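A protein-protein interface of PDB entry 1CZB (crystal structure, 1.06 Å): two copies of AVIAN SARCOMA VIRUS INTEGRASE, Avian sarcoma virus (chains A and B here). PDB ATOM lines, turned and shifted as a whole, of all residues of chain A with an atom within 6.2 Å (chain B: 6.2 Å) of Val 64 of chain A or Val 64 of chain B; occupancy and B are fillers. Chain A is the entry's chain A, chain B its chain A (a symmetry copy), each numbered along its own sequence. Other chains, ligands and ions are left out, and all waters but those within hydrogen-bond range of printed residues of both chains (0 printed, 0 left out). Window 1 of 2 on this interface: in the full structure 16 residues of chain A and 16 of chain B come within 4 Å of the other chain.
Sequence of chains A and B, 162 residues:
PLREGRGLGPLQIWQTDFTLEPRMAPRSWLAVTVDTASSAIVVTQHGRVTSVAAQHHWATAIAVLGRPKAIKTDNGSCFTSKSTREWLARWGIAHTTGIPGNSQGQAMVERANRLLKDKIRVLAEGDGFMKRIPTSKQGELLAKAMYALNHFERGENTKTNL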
ATOM      1  N   ILE A  41     -19.339 -10.371   3.857  1.00  0.00           N
ATOM      2  CA  ILE A  41     -19.655  -9.356   4.847  1.00  0.00           C
ATOM      3  C   ILE A  41     -19.044  -8.019   4.419  1.00  0.00           C
ATOM      4  O   ILE A  41     -17.866  -7.949   4.033  1.00  0.00           O
ATOM      5  CB  ILE A  41     -19.177  -9.874   6.212  1.00  0.00           C
ATOM      6  CG1 ILE A  41     -19.954 -11.136   6.663  1.00  0.00           C
ATOM      7  CG2 ILE A  41     -19.237  -8.766   7.246  1.00  0.00           C
ATOM      8  CD1 ILE A  41     -19.290 -11.822   7.844  1.00  0.00           C
ATOM      9  N   VAL A  42     -19.796  -6.950   4.562  1.00  0.00           N
ATOM     10  CA  VAL A  42     -19.261  -5.581   4.489  1.00  0.00           C
ATOM     11  C   VAL A  42     -19.562  -4.921   5.828  1.00  0.00           C
ATOM     12  O   VAL A  42     -20.705  -4.966   6.290  1.00  0.00           O
ATOM     13  CB  VAL A  42     -19.892  -4.765   3.344  1.00  0.00           C
ATOM     14  CG1 VAL A  42     -19.377  -3.361   3.335  1.00  0.00           C
ATOM     15  CG2 VAL A  42     -19.640  -5.440   2.004  1.00  0.00           C
ATOM     16  N   ALA A  59     -24.083   2.597   0.589  1.00  0.00           N
ATOM     17  CA  ALA A  59     -23.319   3.130  -0.554  1.00  0.00           C
ATOM     18  C   ALA A  59     -22.006   2.366  -0.673  1.00  0.00           C
ATOM     19  O   ALA A  59     -21.561   1.978  -1.758  1.00  0.00           O
ATOM     20  CB  ALA A  59     -23.135   4.621  -0.419  1.00  0.00           C
ATOM     21  N   THR A  60     -21.303   2.187   0.456  1.00  0.00           N
ATOM     22  CA  THR A  60     -20.070   1.415   0.481  1.00  0.00           C
ATOM     23  C   THR A  60     -20.314  -0.038   0.070  1.00  0.00           C
ATOM     24  O   THR A  60     -19.555  -0.596  -0.732  1.00  0.00           O
ATOM     25  CB  THR A  60     -19.426   1.498   1.866  1.00  0.00           C
ATOM     26  OG1 THR A  60     -19.170   2.855   2.154  1.00  0.00           O
ATOM     27  CG2 THR A  60     -18.172   0.641   1.946  1.00  0.00           C
ATOM     28  N   ALA A  61     -21.340  -0.667   0.631  1.00  0.00           N
ATOM     29  CA  ALA A  61     -21.611  -2.050   0.321  1.00  0.00           C
ATOM     30  C   ALA A  61     -21.897  -2.255  -1.159  1.00  0.00           C
ATOM     31  O   ALA A  61     -21.474  -3.259  -1.727  1.00  0.00           O
ATOM     32  CB  ALA A  61     -22.729  -2.608   1.196  1.00  0.00           C
ATOM     33  N   ILE A  62     -22.608  -1.333  -1.797  1.00  0.00           N
ATOM     34  CA  ILE A  62     -22.881  -1.412  -3.240  1.00  0.00           C
ATOM     35  C   ILE A  62     -21.600  -1.303  -4.007  1.00  0.00           C
ATOM     36  O   ILE A  62     -21.397  -2.039  -4.990  1.00  0.00           O
ATOM     37  CB  ILE A  62     -23.893  -0.342  -3.653  1.00  0.00           C
ATOM     38  CG1 ILE A  62     -25.276  -0.621  -3.028  1.00  0.00           C
ATOM     39  CG2 ILE A  62     -24.001  -0.176  -5.143  1.00  0.00           C
ATOM     40  CD1 ILE A  62     -26.226   0.595  -3.124  1.00  0.00           C
ATOM     41  N   ALA A  63     -20.690  -0.428  -3.628  1.00  0.00           N
ATOM     42  CA  ALA A  63     -19.361  -0.328  -4.263  1.00  0.00           C
ATOM     43  C   ALA A  63     -18.622  -1.646  -4.188  1.00  0.00           C
ATOM     44  O   ALA A  63     -17.912  -2.024  -5.121  1.00  0.00           O
ATOM     45  CB  ALA A  63     -18.554   0.790  -3.681  1.00  0.00           C
ATOM     46  N   VAL A  64     -18.726  -2.321  -3.055  1.00  0.00           N
ATOM     47  CA  VAL A  64     -17.985  -3.587  -2.849  1.00  0.00           C
ATOM     48  C   VAL A  64     -18.648  -4.773  -3.526  1.00  0.00           C
ATOM     49  O   VAL A  64     -17.975  -5.561  -4.186  1.00  0.00           O
ATOM     50  CB  VAL A  64     -17.805  -3.837  -1.346  1.00  0.00           C
ATOM     51  CG1 VAL A  64     -17.210  -5.224  -1.088  1.00  0.00           C
ATOM     52  CG2 VAL A  64     -17.012  -2.726  -0.751  1.00  0.00           C
ATOM     53  N   LEU A  65     -19.954  -4.935  -3.330  1.00  0.00           N
ATOM     54  CA  LEU A  65     -20.681  -6.125  -3.748  1.00  0.00           C
ATOM     55  C   LEU A  65     -21.507  -5.987  -4.993  1.00  0.00           C
ATOM     56  O   LEU A  65     -21.969  -7.014  -5.536  1.00  0.00           O
ATOM     57  CB  LEU A  65     -21.647  -6.485  -2.617  1.00  0.00           C
ATOM     58  CG  LEU A  65     -21.033  -6.874  -1.265  1.00  0.00           C
ATOM     59  CD1 LEU A  65     -22.115  -7.037  -0.231  1.00  0.00           C
ATOM     60  CD2 LEU A  65     -20.125  -8.102  -1.463  1.00  0.00           C
ATOM     61  N   GLY A  66     -21.807  -4.815  -5.450  1.00  0.00           N
ATOM     62  CA  GLY A  66     -22.783  -4.613  -6.517  1.00  0.00           C
ATOM     63  C   GLY A  66     -24.126  -4.228  -5.890  1.00  0.00           C
ATOM     64  O   GLY A  66     -24.322  -4.209  -4.687  1.00  0.00           O
ATOM     65  N   MET A 146     -12.718  -7.606   8.385  1.00  0.00           N
ATOM     66  CA  MET A 146     -13.521  -7.887   7.234  1.00  0.00           C
ATOM     67  C   MET A 146     -12.804  -8.835   6.275  1.00  0.00           C
ATOM     68  O   MET A 146     -13.391  -9.821   5.802  1.00  0.00           O
ATOM     69  CB  MET A 146     -13.882  -6.577   6.521  1.00  0.00           C
ATOM     70  CG  MET A 146     -14.740  -6.756   5.290  1.00  0.00           C
ATOM     71  SD  MET A 146     -15.291  -5.161   4.663  1.00  0.00           S
ATOM     72  CE  MET A 146     -15.629  -5.618   2.950  1.00  0.00           C
ATOM     73  N   HIS A 151     -12.199 -13.696   2.926  1.00  0.00           N
ATOM     74  CA  HIS A 151     -11.224 -14.104   1.918  1.00  0.00           C
ATOM     75  C   HIS A 151     -10.511 -15.305   2.465  1.00  0.00           C
ATOM     76  O   HIS A 151      -9.792 -15.168   3.447  1.00  0.00           O
ATOM     77  CB  HIS A 151     -10.267 -12.933   1.561  1.00  0.00           C
ATOM     78  CG  HIS A 151     -11.041 -11.812   0.923  1.00  0.00           C
ATOM     79  ND1 HIS A 151     -11.668 -11.961  -0.318  1.00  0.00           N
ATOM     80  CD2 HIS A 151     -11.303 -10.501   1.350  1.00  0.00           C
ATOM     81  CE1 HIS A 151     -12.276 -10.832  -0.634  1.00  0.00           C
ATOM     82  NE2 HIS A 151     -12.065  -9.976   0.357  1.00  0.00           N
ATOM     83  N   ILE B  41     -11.688  -2.069  -9.624  1.00  0.00           N
ATOM     84  CA  ILE B  41     -11.092  -0.860  -9.084  1.00  0.00           C
ATOM     85  C   ILE B  41     -11.513  -0.692  -7.622  1.00  0.00           C
ATOM     86  O   ILE B  41     -12.699  -0.824  -7.280  1.00  0.00           O
ATOM     87  CB  ILE B  41     -11.488   0.305 -10.006  1.00  0.00           C
ATOM     88  CG1 ILE B  41     -10.889   0.155 -11.426  1.00  0.00           C
ATOM     89  CG2 ILE B  41     -11.121   1.630  -9.366  1.00  0.00           C
ATOM     90  CD1 ILE B  41     -11.517   1.123 -12.414  1.00  0.00           C
ATOM     91  N   VAL B  42     -10.579  -0.320  -6.774  1.00  0.00           N
ATOM     92  CA  VAL B  42     -10.878   0.174  -5.421  1.00  0.00           C
ATOM     93  C   VAL B  42     -10.316   1.586  -5.335  1.00  0.00           C
ATOM     94  O   VAL B  42      -9.150   1.804  -5.679  1.00  0.00           O
ATOM     95  CB  VAL B  42     -10.256  -0.711  -4.323  1.00  0.00           C
ATOM     96  CG1 VAL B  42     -10.523  -0.150  -2.963  1.00  0.00           C
ATOM     97  CG2 VAL B  42     -10.773  -2.138  -4.429  1.00  0.00           C
ATOM     98  N   ALA B  59      -5.227  -1.438   2.993  1.00  0.00           N
ATOM     99  CA  ALA B  59      -6.017  -2.180   3.993  1.00  0.00           C
ATOM    100  C   ALA B  59      -7.446  -2.330   3.483  1.00  0.00           C
ATOM    101  O   ALA B  59      -8.074  -3.390   3.573  1.00  0.00           O
ATOM    102  CB  ALA B  59      -5.929  -1.512   5.341  1.00  0.00           C
ATOM    103  N   THR B  60      -8.032  -1.229   2.987  1.00  0.00           N
ATOM    104  CA  THR B  60      -9.367  -1.262   2.409  1.00  0.00           C
ATOM    105  C   THR B  60      -9.423  -2.183   1.189  1.00  0.00           C
ATOM    106  O   THR B  60     -10.354  -2.986   1.055  1.00  0.00           O
ATOM    107  CB  THR B  60      -9.822   0.155   2.056  1.00  0.00           C
ATOM    108  OG1 THR B  60      -9.809   0.931   3.234  1.00  0.00           O
ATOM    109  CG2 THR B  60     -11.185   0.147   1.382  1.00  0.00           C
ATOM    110  N   ALA B  61      -8.460  -2.055   0.284  1.00  0.00           N
ATOM    111  CA  ALA B  61      -8.465  -2.862  -0.912  1.00  0.00           C
ATOM    112  C   ALA B  61      -8.394  -4.348  -0.595  1.00  0.00           C
ATOM    113  O   ALA B  61      -9.044  -5.146  -1.266  1.00  0.00           O
ATOM    114  CB  ALA B  61      -7.364  -2.435  -1.878  1.00  0.00           C
ATOM    115  N   ILE B  62      -7.615  -4.741   0.406  1.00  0.00           N
ATOM    116  CA  ILE B  62      -7.530  -6.147   0.828  1.00  0.00           C
ATOM    117  C   ILE B  62      -8.855  -6.601   1.358  1.00  0.00           C
ATOM    118  O   ILE B  62      -9.293  -7.727   1.061  1.00  0.00           O
ATOM    119  CB  ILE B  62      -6.407  -6.333   1.849  1.00  0.00           C
ATOM    120  CG1 ILE B  62      -5.028  -6.086   1.202  1.00  0.00           C
ATOM    121  CG2 ILE B  62      -6.446  -7.670   2.534  1.00  0.00           C
ATOM    122  CD1 ILE B  62      -3.903  -5.918   2.250  1.00  0.00           C
ATOM    123  N   ALA B  63      -9.552  -5.796   2.134  1.00  0.00           N
ATOM    124  CA  ALA B  63     -10.910  -6.123   2.614  1.00  0.00           C
ATOM    125  C   ALA B  63     -11.848  -6.381   1.455  1.00  0.00           C
ATOM    126  O   ALA B  63     -12.716  -7.252   1.529  1.00  0.00           O
ATOM    127  CB  ALA B  63     -11.442  -5.064   3.528  1.00  0.00           C
ATOM    128  N   VAL B  64     -11.728  -5.584   0.406  1.00  0.00           N
ATOM    129  CA  VAL B  64     -12.644  -5.702  -0.752  1.00  0.00           C
ATOM    130  C   VAL B  64     -12.276  -6.848  -1.678  1.00  0.00           C
ATOM    131  O   VAL B  64     -13.145  -7.614  -2.087  1.00  0.00           O
ATOM    132  CB  VAL B  64     -12.687  -4.370  -1.511  1.00  0.00           C
ATOM    133  CG1 VAL B  64     -13.476  -4.507  -2.817  1.00  0.00           C
ATOM    134  CG2 VAL B  64     -13.206  -3.304  -0.609  1.00  0.00           C
ATOM    135  N   LEU B  65     -11.002  -6.944  -2.052  1.00  0.00           N
ATOM    136  CA  LEU B  65     -10.542  -7.863  -3.083  1.00  0.00           C
ATOM    137  C   LEU B  65      -9.855  -9.106  -2.598  1.00  0.00           C
ATOM    138  O   LEU B  65      -9.640 -10.038  -3.402  1.00  0.00           O
ATOM    139  CB  LEU B  65      -9.526  -7.105  -3.941  1.00  0.00           C
ATOM    140  CG  LEU B  65     -10.035  -5.886  -4.722  1.00  0.00           C
ATOM    141  CD1 LEU B  65      -8.883  -5.170  -5.377  1.00  0.00           C
ATOM    142  CD2 LEU B  65     -11.155  -6.337  -5.678  1.00  0.00           C
ATOM    143  N   GLY B  66      -9.416  -9.176  -1.383  1.00  0.00           N
ATOM    144  CA  GLY B  66      -8.551 -10.258  -0.920  1.00  0.00           C
ATOM    145  C   GLY B  66      -7.098  -9.774  -0.951  1.00  0.00           C
ATOM    146  O   GLY B  66      -6.763  -8.690  -1.395  1.00  0.00           O
ATOM    147  N   MET B 146     -17.170   4.187  -7.951  1.00  0.00           N
ATOM    148  CA  MET B 146     -16.567   2.891  -7.884  1.00  0.00           C
ATOM    149  C   MET B 146     -17.541   1.800  -8.326  1.00  0.00           C
ATOM    150  O   MET B 146     -17.189   0.926  -9.132  1.00  0.00           O
ATOM    151  CB  MET B 146     -16.074   2.621  -6.455  1.00  0.00           C
ATOM    152  CG  MET B 146     -15.409   1.277  -6.272  1.00  0.00           C
ATOM    153  SD  MET B 146     -14.671   1.152  -4.634  1.00  0.00           S
ATOM    154  CE  MET B 146     -14.618  -0.644  -4.471  1.00  0.00           C
ATOM    155  N   HIS B 151     -19.348  -2.860 -11.523  1.00  0.00           N
ATOM    156  CA  HIS B 151     -20.489  -3.766 -11.418  1.00  0.00           C
ATOM    157  C   HIS B 151     -21.327  -3.553 -12.644  1.00  0.00           C
ATOM    158  O   HIS B 151     -21.893  -2.476 -12.792  1.00  0.00           O
ATOM    159  CB  HIS B 151     -21.268  -3.531 -10.095  1.00  0.00           C
ATOM    160  CG  HIS B 151     -20.395  -3.866  -8.917  1.00  0.00           C
ATOM    161  ND1 HIS B 151     -19.952  -5.170  -8.674  1.00  0.00           N
ATOM    162  CD2 HIS B 151     -19.867  -3.066  -7.892  1.00  0.00           C
ATOM    163  CE1 HIS B 151     -19.202  -5.177  -7.587  1.00  0.00           C
ATOM    164  NE2 HIS B 151     -19.148  -3.932  -7.134  1.00  0.00           N
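Of the 12 printed residues of chain A, 7 touch a printed residue of chain B. Hydrophobic or aromatic side chains of chain A within 4 Å of the printed part of chain B: Val 64, Met 146 and His 151. Along chain A the printed residues that touch a printed residue of chain B span positions 62 to 151. Among the printed residues, no Asp or Glu carboxylate lies within 4 Å of a Lys or Arg side-chain nitrogen of the other chain.
Ala 63 of chain A touches Met 146 of chain B, and with the chains exchanged Met 146 of chain A touches Ala 63 of chain B. Ala 63 of chain A touches His 151 of chain B, and with the chains exchanged His 151 of chain A touches Ala 63 of chain B. Val 64 of chain A touches His 151 of chain B, and with the chains exchanged His 151 of chain A touches Val 64 of chain B. Leu 65 of chain A touches His 151 of chain B, and with the chains exchanged His 151 of chain A touches Leu 65 of chain B. Of the 13 pairs that touch across the chains among the printed residues, 13 have their exchanged pair printed and touching as well.
Among the printed residues, pairs that only touch across the chains: Ile 62 of chain A with His 151 of chain B (3.4 Å), Ala 63 of chain A with Met 146 of chain B (3.6 Å), Val 64 of chain A with Val 64 of chain B (3.9 Å), Val 64 of chain A with His 151 of chain B (3.6 Å), Leu 65 of chain A with His 151 of chain B (3.6 Å), Met 146 of chain A with Ala 63 of chain B (3.6 Å), His 151 of chain A with Ile 62 of chain B (3.4 Å), His 151 of chain A with Val 64 of chain B (3.6 Å) and His 151 of chain A with Leu 65 of chain B (3.6 Å).
Val 64 of chain A touches just these residues of chain B: Val 64 and His 151. Val 64 of chain B touches two residues of chain A. Of the printed residues of chain A, Leu 65 of chain B touches His 151 (3.6 Å). Of the printed residues of chain A, Met 146 of chain B touches Ala 63 (3.6 Å). Printed residues of chain A within 4 Å of Ala 63 of chain B: Met 146 (3.6 Å) and His 151 (3.0 Å). Printed residues of chain B within 4 Å of Ile 62 of chain A: His 151. Of the printed residues of chain B, Ala 63 of chain A touches Met 146 (3.6 Å) and His 151 (3.0 Å). The nearest printed residue of chain A that does not touch Leu 65 of chain B is Val 64 of chain A (6.5 Å).
A ring nitrogen (NE2) of His 151 of chain B sits at hydrogen-bond distance from the backbone carbonyl oxygen (O) of Ala 63 of chain A. A ring nitrogen (NE2) of His 151 of chain B sits at hydrogen-bond distance from the backbone NH (N) of Gly 66 of chain A, 3.3 Å away. NE2 of His 151 of chain A sits at hydrogen-bond distance from O of Ala 63 of chain B, 3.0 Å away. The backbone NH (N) of Gly 66 of chain B lies within hydrogen-bond range of a ring nitrogen (NE2) of His 151 of chain A (3.3 Å).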
